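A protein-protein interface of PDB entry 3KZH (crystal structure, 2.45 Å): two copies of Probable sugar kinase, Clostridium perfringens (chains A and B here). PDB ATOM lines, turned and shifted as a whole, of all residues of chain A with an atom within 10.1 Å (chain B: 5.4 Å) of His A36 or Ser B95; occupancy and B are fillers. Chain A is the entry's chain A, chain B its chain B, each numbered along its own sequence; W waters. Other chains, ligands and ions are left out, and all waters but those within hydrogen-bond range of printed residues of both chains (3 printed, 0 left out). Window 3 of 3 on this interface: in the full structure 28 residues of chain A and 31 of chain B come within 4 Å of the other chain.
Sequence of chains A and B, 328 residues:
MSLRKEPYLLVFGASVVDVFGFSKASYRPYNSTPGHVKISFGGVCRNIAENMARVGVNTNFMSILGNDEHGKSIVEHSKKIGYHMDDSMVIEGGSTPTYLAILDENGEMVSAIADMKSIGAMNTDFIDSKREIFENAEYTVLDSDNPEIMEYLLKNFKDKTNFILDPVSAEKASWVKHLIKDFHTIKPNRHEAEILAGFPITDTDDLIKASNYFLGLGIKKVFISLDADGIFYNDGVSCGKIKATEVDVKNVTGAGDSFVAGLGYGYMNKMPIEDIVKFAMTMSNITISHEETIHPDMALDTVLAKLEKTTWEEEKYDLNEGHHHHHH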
ATOM      1  N   ASP A  18      -6.914 -13.970 -23.259  1.00  0.00           N
ATOM      2  CA  ASP A  18      -6.504 -13.758 -21.867  1.00  0.00           C
ATOM      3  C   ASP A  18      -5.135 -13.064 -21.801  1.00  0.00           C
ATOM      4  O   ASP A  18      -4.201 -13.463 -22.493  1.00  0.00           O
ATOM      5  CB  ASP A  18      -6.421 -15.088 -21.116  1.00  0.00           C
ATOM      6  CG  ASP A  18      -7.782 -15.693 -20.816  1.00  0.00           C
ATOM      7  OD1 ASP A  18      -8.707 -14.957 -20.426  1.00  0.00           O
ATOM      8  OD2 ASP A  18      -7.914 -16.927 -20.935  1.00  0.00           O
ATOM      9  N   VAL A  19      -5.051 -11.979 -21.029  1.00  0.00           N
ATOM     10  CA  VAL A  19      -3.801 -11.221 -20.841  1.00  0.00           C
ATOM     11  C   VAL A  19      -3.502 -11.219 -19.336  1.00  0.00           C
ATOM     12  O   VAL A  19      -4.164 -10.535 -18.557  1.00  0.00           O
ATOM     13  CB  VAL A  19      -3.897  -9.758 -21.390  1.00  0.00           C
ATOM     14  CG1 VAL A  19      -2.514  -9.106 -21.398  1.00  0.00           C
ATOM     15  CG2 VAL A  19      -4.476  -9.730 -22.809  1.00  0.00           C
ATOM     16  N   PHE A  20      -2.517 -12.018 -18.944  1.00  0.00           N
ATOM     17  CA  PHE A  20      -2.134 -12.175 -17.545  1.00  0.00           C
ATOM     18  C   PHE A  20      -0.784 -11.564 -17.182  1.00  0.00           C
ATOM     19  O   PHE A  20       0.219 -11.819 -17.849  1.00  0.00           O
ATOM     20  CB  PHE A  20      -2.102 -13.661 -17.171  1.00  0.00           C
ATOM     21  CG  PHE A  20      -3.453 -14.313 -17.067  1.00  0.00           C
ATOM     22  CD1 PHE A  20      -4.366 -13.927 -16.069  1.00  0.00           C
ATOM     23  CD2 PHE A  20      -3.794 -15.379 -17.929  1.00  0.00           C
ATOM     24  CE1 PHE A  20      -5.618 -14.594 -15.915  1.00  0.00           C
ATOM     25  CE2 PHE A  20      -5.043 -16.062 -17.792  1.00  0.00           C
ATOM     26  CZ  PHE A  20      -5.957 -15.665 -16.779  1.00  0.00           C
ATOM     27  N   GLY A  21      -0.769 -10.785 -16.102  1.00  0.00           N
ATOM     28  CA  GLY A  21       0.457 -10.171 -15.617  1.00  0.00           C
ATOM     29  C   GLY A  21       0.844 -10.789 -14.290  1.00  0.00           C
ATOM     30  O   GLY A  21       0.125 -10.633 -13.306  1.00  0.00           O
ATOM     31  N   PHE A  22       1.954 -11.526 -14.278  1.00  0.00           N
ATOM     32  CA  PHE A  22       2.455 -12.194 -13.073  1.00  0.00           C
ATOM     33  C   PHE A  22       3.546 -11.347 -12.426  1.00  0.00           C
ATOM     34  O   PHE A  22       4.565 -11.079 -13.061  1.00  0.00           O
ATOM     35  CB  PHE A  22       3.045 -13.574 -13.419  1.00  0.00           C
ATOM     36  CG  PHE A  22       2.064 -14.529 -14.044  1.00  0.00           C
ATOM     37  CD1 PHE A  22       1.387 -15.482 -13.253  1.00  0.00           C
ATOM     38  CD2 PHE A  22       1.814 -14.499 -15.434  1.00  0.00           C
ATOM     39  CE1 PHE A  22       0.462 -16.401 -13.838  1.00  0.00           C
ATOM     40  CE2 PHE A  22       0.898 -15.408 -16.028  1.00  0.00           C
ATOM     41  CZ  PHE A  22       0.220 -16.361 -15.227  1.00  0.00           C
ATOM     42  N   SER A  23       3.351 -10.964 -11.162  1.00  0.00           N
ATOM     43  CA  SER A  23       4.331 -10.152 -10.424  1.00  0.00           C
ATOM     44  C   SER A  23       5.621 -10.913 -10.103  1.00  0.00           C
ATOM     45  O   SER A  23       5.569 -12.036  -9.601  1.00  0.00           O
ATOM     46  CB  SER A  23       3.735  -9.618  -9.112  1.00  0.00           C
ATOM     47  OG  SER A  23       2.687  -8.690  -9.313  1.00  0.00           O
ATOM     48  N   LYS A  24       6.762 -10.300 -10.442  1.00  0.00           N
ATOM     49  CA  LYS A  24       8.098 -10.867 -10.185  1.00  0.00           C
ATOM     50  C   LYS A  24       8.803 -10.117  -9.041  1.00  0.00           C
ATOM     51  O   LYS A  24      10.025 -10.174  -8.880  1.00  0.00           O
ATOM     52  CB  LYS A  24       8.953 -10.865 -11.466  1.00  0.00           C
ATOM     53  CG  LYS A  24       8.498 -11.862 -12.543  1.00  0.00           C
ATOM     54  CD  LYS A  24       8.610 -13.304 -12.061  1.00  0.00           C
ATOM     55  CE  LYS A  24       7.978 -14.270 -13.031  1.00  0.00           C
ATOM     56  NZ  LYS A  24       8.065 -15.664 -12.513  1.00  0.00           N
ATOM     57  N   ALA A  25       7.991  -9.400  -8.273  1.00  0.00           N
ATOM     58  CA  ALA A  25       8.392  -8.624  -7.105  1.00  0.00           C
ATOM     59  C   ALA A  25       7.127  -8.447  -6.281  1.00  0.00           C
ATOM     60  O   ALA A  25       6.021  -8.641  -6.810  1.00  0.00           O
ATOM     61  CB  ALA A  25       8.927  -7.270  -7.502  1.00  0.00           C
ATOM     62  N   THR A  33       4.521  -2.640 -10.732  1.00  0.00           N
ATOM     63  CA  THR A  33       5.253  -3.828 -10.280  1.00  0.00           C
ATOM     64  C   THR A  33       5.951  -4.537 -11.455  1.00  0.00           C
ATOM     65  O   THR A  33       5.346  -4.705 -12.509  1.00  0.00           O
ATOM     66  CB  THR A  33       4.285  -4.865  -9.614  1.00  0.00           C
ATOM     67  OG1 THR A  33       3.415  -4.203  -8.690  1.00  0.00           O
ATOM     68  CG2 THR A  33       5.059  -5.947  -8.867  1.00  0.00           C
ATOM     69  N   PRO A  34       7.244  -4.915 -11.312  1.00  0.00           N
ATOM     70  CA  PRO A  34       7.882  -5.608 -12.441  1.00  0.00           C
ATOM     71  C   PRO A  34       7.344  -7.038 -12.566  1.00  0.00           C
ATOM     72  O   PRO A  34       7.106  -7.710 -11.553  1.00  0.00           O
ATOM     73  CB  PRO A  34       9.370  -5.570 -12.078  1.00  0.00           C
ATOM     74  CG  PRO A  34       9.365  -5.492 -10.607  1.00  0.00           C
ATOM     75  CD  PRO A  34       8.262  -4.519 -10.324  1.00  0.00           C
ATOM     76  N   GLY A  35       7.074  -7.458 -13.797  1.00  0.00           N
ATOM     77  CA  GLY A  35       6.539  -8.787 -13.994  1.00  0.00           C
ATOM     78  C   GLY A  35       6.632  -9.394 -15.375  1.00  0.00           C
ATOM     79  O   GLY A  35       7.385  -8.931 -16.228  1.00  0.00           O
ATOM     80  N   HIS A  36       5.866 -10.464 -15.563  1.00  0.00           N
ATOM     81  CA  HIS A  36       5.825 -11.195 -16.817  1.00  0.00           C
ATOM     82  C   HIS A  36       4.411 -11.237 -17.380  1.00  0.00           C
ATOM     83  O   HIS A  36       3.479 -11.661 -16.698  1.00  0.00           O
ATOM     84  CB  HIS A  36       6.372 -12.617 -16.621  1.00  0.00           C
ATOM     85  CG  HIS A  36       6.473 -13.409 -17.888  1.00  0.00           C
ATOM     86  ND1 HIS A  36       7.080 -12.917 -19.023  1.00  0.00           N
ATOM     87  CD2 HIS A  36       6.029 -14.646 -18.203  1.00  0.00           C
ATOM     88  CE1 HIS A  36       7.006 -13.821 -19.982  1.00  0.00           C
ATOM     89  NE2 HIS A  36       6.375 -14.880 -19.512  1.00  0.00           N
ATOM     90  N   VAL A  37       4.282 -10.805 -18.630  1.00  0.00           N
ATOM     91  CA  VAL A  37       3.007 -10.790 -19.337  1.00  0.00           C
ATOM     92  C   VAL A  37       2.850 -12.040 -20.208  1.00  0.00           C
ATOM     93  O   VAL A  37       3.730 -12.369 -21.010  1.00  0.00           O
ATOM     94  CB  VAL A  37       2.849  -9.525 -20.203  1.00  0.00           C
ATOM     95  CG1 VAL A  37       1.480  -9.501 -20.904  1.00  0.00           C
ATOM     96  CG2 VAL A  37       3.007  -8.308 -19.347  1.00  0.00           C
ATOM     97  N   LYS A  38       1.715 -12.712 -20.039  1.00  0.00           N
ATOM     98  CA  LYS A  38       1.392 -13.925 -20.780  1.00  0.00           C
ATOM     99  C   LYS A  38       0.082 -13.689 -21.537  1.00  0.00           C
ATOM    100  O   LYS A  38      -0.916 -13.265 -20.957  1.00  0.00           O
ATOM    101  CB  LYS A  38       1.247 -15.101 -19.797  1.00  0.00           C
ATOM    102  CG  LYS A  38       1.721 -16.462 -20.292  1.00  0.00           C
ATOM    103  CD  LYS A  38       0.676 -17.197 -21.135  1.00  0.00           C
ATOM    104  CE  LYS A  38       1.302 -18.348 -21.917  1.00  0.00           C
ATOM    105  NZ  LYS A  38       0.405 -18.859 -22.997  1.00  0.00           N
ATOM    106  N   ILE A  39       0.123 -13.912 -22.848  1.00  0.00           N
ATOM    107  CA  ILE A  39      -1.054 -13.764 -23.706  1.00  0.00           C
ATOM    108  C   ILE A  39      -1.455 -15.157 -24.202  1.00  0.00           C
ATOM    109  O   ILE A  39      -0.628 -15.897 -24.740  1.00  0.00           O
ATOM    110  CB  ILE A  39      -0.803 -12.832 -24.937  1.00  0.00           C
ATOM    111  CG1 ILE A  39      -0.181 -11.499 -24.514  1.00  0.00           C
ATOM    112  CG2 ILE A  39      -2.118 -12.523 -25.648  1.00  0.00           C
ATOM    113  CD1 ILE A  39       1.345 -11.499 -24.513  1.00  0.00           C
ATOM    114  N   LEU A 100      -8.240  -9.189 -18.811  1.00  0.00           N
ATOM    115  CA  LEU A 100      -6.963  -8.643 -18.361  1.00  0.00           C
ATOM    116  C   LEU A 100      -6.855  -8.802 -16.844  1.00  0.00           C
ATOM    117  O   LEU A 100      -7.637  -8.215 -16.113  1.00  0.00           O
ATOM    118  CB  LEU A 100      -6.858  -7.168 -18.776  1.00  0.00           C
ATOM    119  CG  LEU A 100      -5.724  -6.254 -18.287  1.00  0.00           C
ATOM    120  CD1 LEU A 100      -4.347  -6.806 -18.655  1.00  0.00           C
ATOM    121  CD2 LEU A 100      -5.920  -4.883 -18.894  1.00  0.00           C
ATOM    122  N   ALA A 101      -5.893  -9.599 -16.386  1.00  0.00           N
ATOM    123  CA  ALA A 101      -5.705  -9.820 -14.953  1.00  0.00           C
ATOM    124  C   ALA A 101      -4.281  -9.704 -14.466  1.00  0.00           C
ATOM    125  O   ALA A 101      -3.351 -10.176 -15.112  1.00  0.00           O
ATOM    126  CB  ALA A 101      -6.262 -11.162 -14.537  1.00  0.00           C
ATOM    127  N   ILE A 102      -4.127  -9.084 -13.298  1.00  0.00           N
ATOM    128  CA  ILE A 102      -2.823  -8.917 -12.666  1.00  0.00           C
ATOM    129  C   ILE A 102      -2.776  -9.799 -11.415  1.00  0.00           C
ATOM    130  O   ILE A 102      -3.647  -9.713 -10.547  1.00  0.00           O
ATOM    131  CB  ILE A 102      -2.520  -7.410 -12.365  1.00  0.00           C
ATOM    132  CG1 ILE A 102      -2.231  -6.692 -13.689  1.00  0.00           C
ATOM    133  CG2 ILE A 102      -1.336  -7.260 -11.395  1.00  0.00           C
ATOM    134  CD1 ILE A 102      -2.189  -5.204 -13.622  1.00  0.00           C
ATOM    135  N   LEU A 103      -1.787 -10.691 -11.385  1.00  0.00           N
ATOM    136  CA  LEU A 103      -1.576 -11.616 -10.274  1.00  0.00           C
ATOM    137  C   LEU A 103      -0.387 -11.176  -9.420  1.00  0.00           C
ATOM    138  O   LEU A 103       0.539 -10.530  -9.928  1.00  0.00           O
ATOM    139  CB  LEU A 103      -1.329 -13.051 -10.777  1.00  0.00           C
ATOM    140  CG  LEU A 103      -2.219 -13.812 -11.775  1.00  0.00           C
ATOM    141  CD1 LEU A 103      -3.690 -13.627 -11.488  1.00  0.00           C
ATOM    142  CD2 LEU A 103      -1.918 -13.357 -13.184  1.00  0.00           C
ATOM    143  N   ASP A 104      -0.419 -11.521  -8.129  1.00  0.00           N
ATOM    144  CA  ASP A 104       0.671 -11.178  -7.219  1.00  0.00           C
ATOM    145  C   ASP A 104       1.780 -12.234  -7.226  1.00  0.00           C
ATOM    146  O   ASP A 104       1.730 -13.169  -8.026  1.00  0.00           O
ATOM    147  CB  ASP A 104       0.165 -10.847  -5.790  1.00  0.00           C
ATOM    148  CG  ASP A 104      -0.555 -12.006  -5.082  1.00  0.00           C
ATOM    149  OD1 ASP A 104      -1.175 -11.729  -4.034  1.00  0.00           O
ATOM    150  OD2 ASP A 104      -0.499 -13.171  -5.524  1.00  0.00           O
ATOM    151  N   GLU A 105       2.767 -12.065  -6.345  1.00  0.00           N
ATOM    152  CA  GLU A 105       3.916 -12.970  -6.202  1.00  0.00           C
ATOM    153  C   GLU A 105       3.546 -14.409  -5.809  1.00  0.00           C
ATOM    154  O   GLU A 105       4.322 -15.345  -6.031  1.00  0.00           O
ATOM    155  CB  GLU A 105       4.918 -12.391  -5.184  1.00  0.00           C
ATOM    156  CG  GLU A 105       4.373 -12.169  -3.746  1.00  0.00           C
ATOM    157  CD  GLU A 105       3.769 -10.782  -3.500  1.00  0.00           C
ATOM    158  OE1 GLU A 105       3.240 -10.149  -4.445  1.00  0.00           O
ATOM    159  OE2 GLU A 105       3.830 -10.319  -2.338  1.00  0.00           O
ATOM    160  N   GLU A 292      -0.521 -26.155 -20.152  1.00  0.00           N
ATOM    161  CA  GLU A 292      -1.355 -25.300 -20.984  1.00  0.00           C
ATOM    162  C   GLU A 292      -2.650 -26.006 -21.384  1.00  0.00           C
ATOM    163  O   GLU A 292      -2.733 -27.238 -21.375  1.00  0.00           O
ATOM    164  CB  GLU A 292      -0.589 -24.826 -22.229  1.00  0.00           C
ATOM    165  CG  GLU A 292       0.647 -23.956 -21.947  1.00  0.00           C
ATOM    166  CD  GLU A 292       0.335 -22.652 -21.215  1.00  0.00           C
ATOM    167  OE1 GLU A 292      -0.529 -21.882 -21.689  1.00  0.00           O
ATOM    168  OE2 GLU A 292       0.961 -22.394 -20.168  1.00  0.00           O
ATOM    169  N   LEU B  65      11.985  -7.822 -29.750  1.00  0.00           N
ATOM    170  CA  LEU B  65      10.660  -8.423 -29.652  1.00  0.00           C
ATOM    171  C   LEU B  65      10.764  -9.856 -29.182  1.00  0.00           C
ATOM    172  O   LEU B  65      11.833 -10.458 -29.229  1.00  0.00           O
ATOM    173  CB  LEU B  65       9.971  -8.434 -31.015  1.00  0.00           C
ATOM    174  CG  LEU B  65       9.591  -7.156 -31.746  1.00  0.00           C
ATOM    175  CD1 LEU B  65       9.027  -7.544 -33.065  1.00  0.00           C
ATOM    176  CD2 LEU B  65       8.602  -6.338 -30.953  1.00  0.00           C
ATOM    177  N   GLY B  66       9.641 -10.382 -28.710  1.00  0.00           N
ATOM    178  CA  GLY B  66       9.570 -11.769 -28.285  1.00  0.00           C
ATOM    179  C   GLY B  66       8.714 -12.503 -29.303  1.00  0.00           C
ATOM    180  O   GLY B  66       8.123 -11.862 -30.173  1.00  0.00           O
ATOM    181  N   ASP B  68       5.857 -13.872 -28.936  1.00  0.00           N
ATOM    182  CA  ASP B  68       4.530 -13.978 -28.339  1.00  0.00           C
ATOM    183  C   ASP B  68       3.528 -13.269 -29.249  1.00  0.00           C
ATOM    184  O   ASP B  68       3.908 -12.788 -30.322  1.00  0.00           O
ATOM    185  CB  ASP B  68       4.508 -13.442 -26.881  1.00  0.00           C
ATOM    186  CG  ASP B  68       4.964 -11.982 -26.748  1.00  0.00           C
ATOM    187  OD1 ASP B  68       5.570 -11.423 -27.692  1.00  0.00           O
ATOM    188  OD2 ASP B  68       4.717 -11.392 -25.671  1.00  0.00           O
ATOM    189  N   ILE B  91      13.505 -12.851 -29.408  1.00  0.00           N
ATOM    190  CA  ILE B  91      13.820 -13.709 -28.271  1.00  0.00           C
ATOM    191  C   ILE B  91      12.798 -14.835 -28.185  1.00  0.00           C
ATOM    192  O   ILE B  91      11.613 -14.603 -27.909  1.00  0.00           O
ATOM    193  CB  ILE B  91      13.872 -12.910 -26.949  1.00  0.00           C
ATOM    194  CG1 ILE B  91      14.886 -11.778 -27.085  1.00  0.00           C
ATOM    195  CG2 ILE B  91      14.312 -13.817 -25.783  1.00  0.00           C
ATOM    196  CD1 ILE B  91      14.772 -10.746 -26.051  1.00  0.00           C
ATOM    197  N   GLY B  93      10.783 -17.679 -26.719  1.00  0.00           N
ATOM    198  CA  GLY B  93      10.266 -17.992 -25.395  1.00  0.00           C
ATOM    199  C   GLY B  93      10.185 -16.781 -24.478  1.00  0.00           C
ATOM    200  O   GLY B  93       9.758 -16.897 -23.326  1.00  0.00           O
ATOM    201  N   GLY B  94      10.623 -15.631 -24.995  1.00  0.00           N
ATOM    202  CA  GLY B  94      10.604 -14.382 -24.251  1.00  0.00           C
ATOM    203  C   GLY B  94       9.425 -13.514 -24.652  1.00  0.00           C
ATOM    204  O   GLY B  94       8.800 -13.723 -25.704  1.00  0.00           O
ATOM    205  N   SER B  95       9.117 -12.536 -23.808  1.00  0.00           N
ATOM    206  CA  SER B  95       8.008 -11.631 -24.067  1.00  0.00           C
ATOM    207  C   SER B  95       8.434 -10.306 -24.680  1.00  0.00           C
ATOM    208  O   SER B  95       9.565  -9.861 -24.515  1.00  0.00           O
ATOM    209  CB  SER B  95       7.227 -11.366 -22.784  1.00  0.00           C
ATOM    210  OG  SER B  95       8.077 -10.887 -21.770  1.00  0.00           O
ATOM    211  N   THR B  96       7.514  -9.709 -25.426  1.00  0.00           N
ATOM    212  CA  THR B  96       7.718  -8.410 -26.048  1.00  0.00           C
ATOM    213  C   THR B  96       7.462  -7.427 -24.903  1.00  0.00           C
ATOM    214  O   THR B  96       6.483  -7.602 -24.174  1.00  0.00           O
ATOM    215  CB  THR B  96       6.707  -8.238 -27.187  1.00  0.00           C
ATOM    216  OG1 THR B  96       7.006  -9.207 -28.193  1.00  0.00           O
ATOM    217  CG2 THR B  96       6.755  -6.856 -27.807  1.00  0.00           C
ATOM    218  N   PRO B  97       8.375  -6.449 -24.666  1.00  0.00           N
ATOM    219  CA  PRO B  97       8.206  -5.466 -23.577  1.00  0.00           C
ATOM    220  C   PRO B  97       6.808  -4.854 -23.521  1.00  0.00           C
ATOM    221  O   PRO B  97       6.314  -4.322 -24.511  1.00  0.00           O
ATOM    222  CB  PRO B  97       9.305  -4.456 -23.867  1.00  0.00           C
ATOM    223  CG  PRO B  97      10.391  -5.350 -24.371  1.00  0.00           C
ATOM    224  CD  PRO B  97       9.661  -6.213 -25.353  1.00  0.00           C
ATOM    225  N   ILE B 113       1.734  -3.725 -14.228  1.00  0.00           N
ATOM    226  CA  ILE B 113       2.834  -4.664 -14.464  1.00  0.00           C
ATOM    227  C   ILE B 113       3.710  -4.150 -15.610  1.00  0.00           C
ATOM    228  O   ILE B 113       3.225  -3.945 -16.728  1.00  0.00           O
ATOM    229  CB  ILE B 113       2.324  -6.124 -14.823  1.00  0.00           C
ATOM    230  CG1 ILE B 113       1.666  -6.817 -13.623  1.00  0.00           C
ATOM    231  CG2 ILE B 113       3.457  -7.011 -15.388  1.00  0.00           C
ATOM    232  CD1 ILE B 113       2.589  -7.302 -12.509  1.00  0.00           C
ATOM    233  N   ASP B 115       6.796  -5.218 -17.846  1.00  0.00           N
ATOM    234  CA  ASP B 115       7.577  -6.374 -18.294  1.00  0.00           C
ATOM    235  C   ASP B 115       8.632  -5.838 -19.241  1.00  0.00           C
ATOM    236  O   ASP B 115       8.392  -5.709 -20.429  1.00  0.00           O
ATOM    237  CB  ASP B 115       6.659  -7.370 -19.020  1.00  0.00           C
ATOM    238  CG  ASP B 115       7.356  -8.674 -19.411  1.00  0.00           C
ATOM    239  OD1 ASP B 115       8.586  -8.830 -19.255  1.00  0.00           O
ATOM    240  OD2 ASP B 115       6.641  -9.565 -19.886  1.00  0.00           O
ATOM    241  N   SER B 118      13.042  -8.256 -21.636  1.00  0.00           N
ATOM    242  CA  SER B 118      13.638  -8.376 -22.961  1.00  0.00           C
ATOM    243  C   SER B 118      14.540  -7.241 -23.452  1.00  0.00           C
ATOM    244  O   SER B 118      15.385  -7.465 -24.316  1.00  0.00           O
ATOM    245  CB  SER B 118      12.564  -8.706 -23.984  1.00  0.00           C
ATOM    246  OG  SER B 118      12.115 -10.031 -23.776  1.00  0.00           O
HETATM  247  O   HOH W   1       6.774 -15.728 -22.829  1.00  0.00           O
HETATM  248  O   HOH W   2       9.289 -11.330 -19.024  1.00  0.00           O
HETATM  249  O   HOH W   3       4.630 -13.235 -23.334  1.00  0.00           O
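The side-chain carboxylate of Asp B115 sits at hydrogen-bond distance from a ring nitrogen (ND1) of His A36.
N of Val A37 lies within hydrogen-bond range of OD2 of Asp B115, at 2.9 Å.
O of Gly A35 lies close to OD1 of Asp B115 (3.3 Å).
N of Phe A22 sits at hydrogen-bond distance from O of His A36 (2.9 Å).
OG of Ser A23 lies within hydrogen-bond range of O of Leu A103, 2.9 Å away.
The side-chain carboxylate of Asp B68 is in hydrogen-bond range of the side-chain hydroxyl of Thr B96 (2.7 Å).
The side-chain carboxylate of Asp B115 is in hydrogen-bond range of the side-chain hydroxyl of Ser B95.
The backbone carbonyl oxygen (O) of Ser B95 is in hydrogen-bond range of the side-chain hydroxyl (OG) of Ser B118.
Among the printed residues, merely in contact across the chains: Ser A23 with Ile B113 (3.5 Å), Thr A33 with Ile B113 (3.2 Å), Gly A35 with Ile B113 (3.8 Å), His A36 with Ser B95 (3.6 Å), Ile A39 with Asp B68 (3.6 Å) and Ile A102 with Ile B113 (3.8 Å).
Of chain B, only Ser B95 and Asp B115 come within 4 Å of His A36.
No residue of chain A comes within 4 Å of Gly B66.
Asp B115 touches three residues of chain A.
Of the printed residues of chain B, Val A37 touches Asp B115.
Of the printed residues of chain B, Thr A33 touches Ile B113 (3.2 Å).
Of the printed residues of chain B, Gly A35 touches Ile B113 and Asp B115.
The nearest printed residue of chain B that does not touch Ile A102 is Asp B115 (9.9 Å).
Of the 12 printed residues of chain B, 4 touch a printed residue of chain A.
Hydrophobic or aromatic side chains of chain B that line the printed part of chain A: Ile B113.
Hydrophobic or aromatic side chains of chain A that line the printed part of chain B: His A36, Val A37, Ile A39 and Ile A102.
Among the printed residues, 9 pairs touch across the chains.
No position is printed for both chains.
Of the 9 pairs that touch across the chains among the printed residues, none has its exchanged pair printed and touching as well.
Water W2 lies within hydrogen-bond range of the side-chain carboxylate of Asp B115 (2.6 Å), a ring nitrogen (ND1) of His A36 (2.7 Å) and the side-chain hydroxyl of Ser B95 (3.0 Å).
Water W3 lies within hydrogen-bond range of the backbone carbonyl oxygen of Val A37 (2.6 Å) and the side-chain carboxylate of Asp B68 (3.0 Å).
Water W1 lies within hydrogen-bond range of O of Gly B93 and NE2 of His A36.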
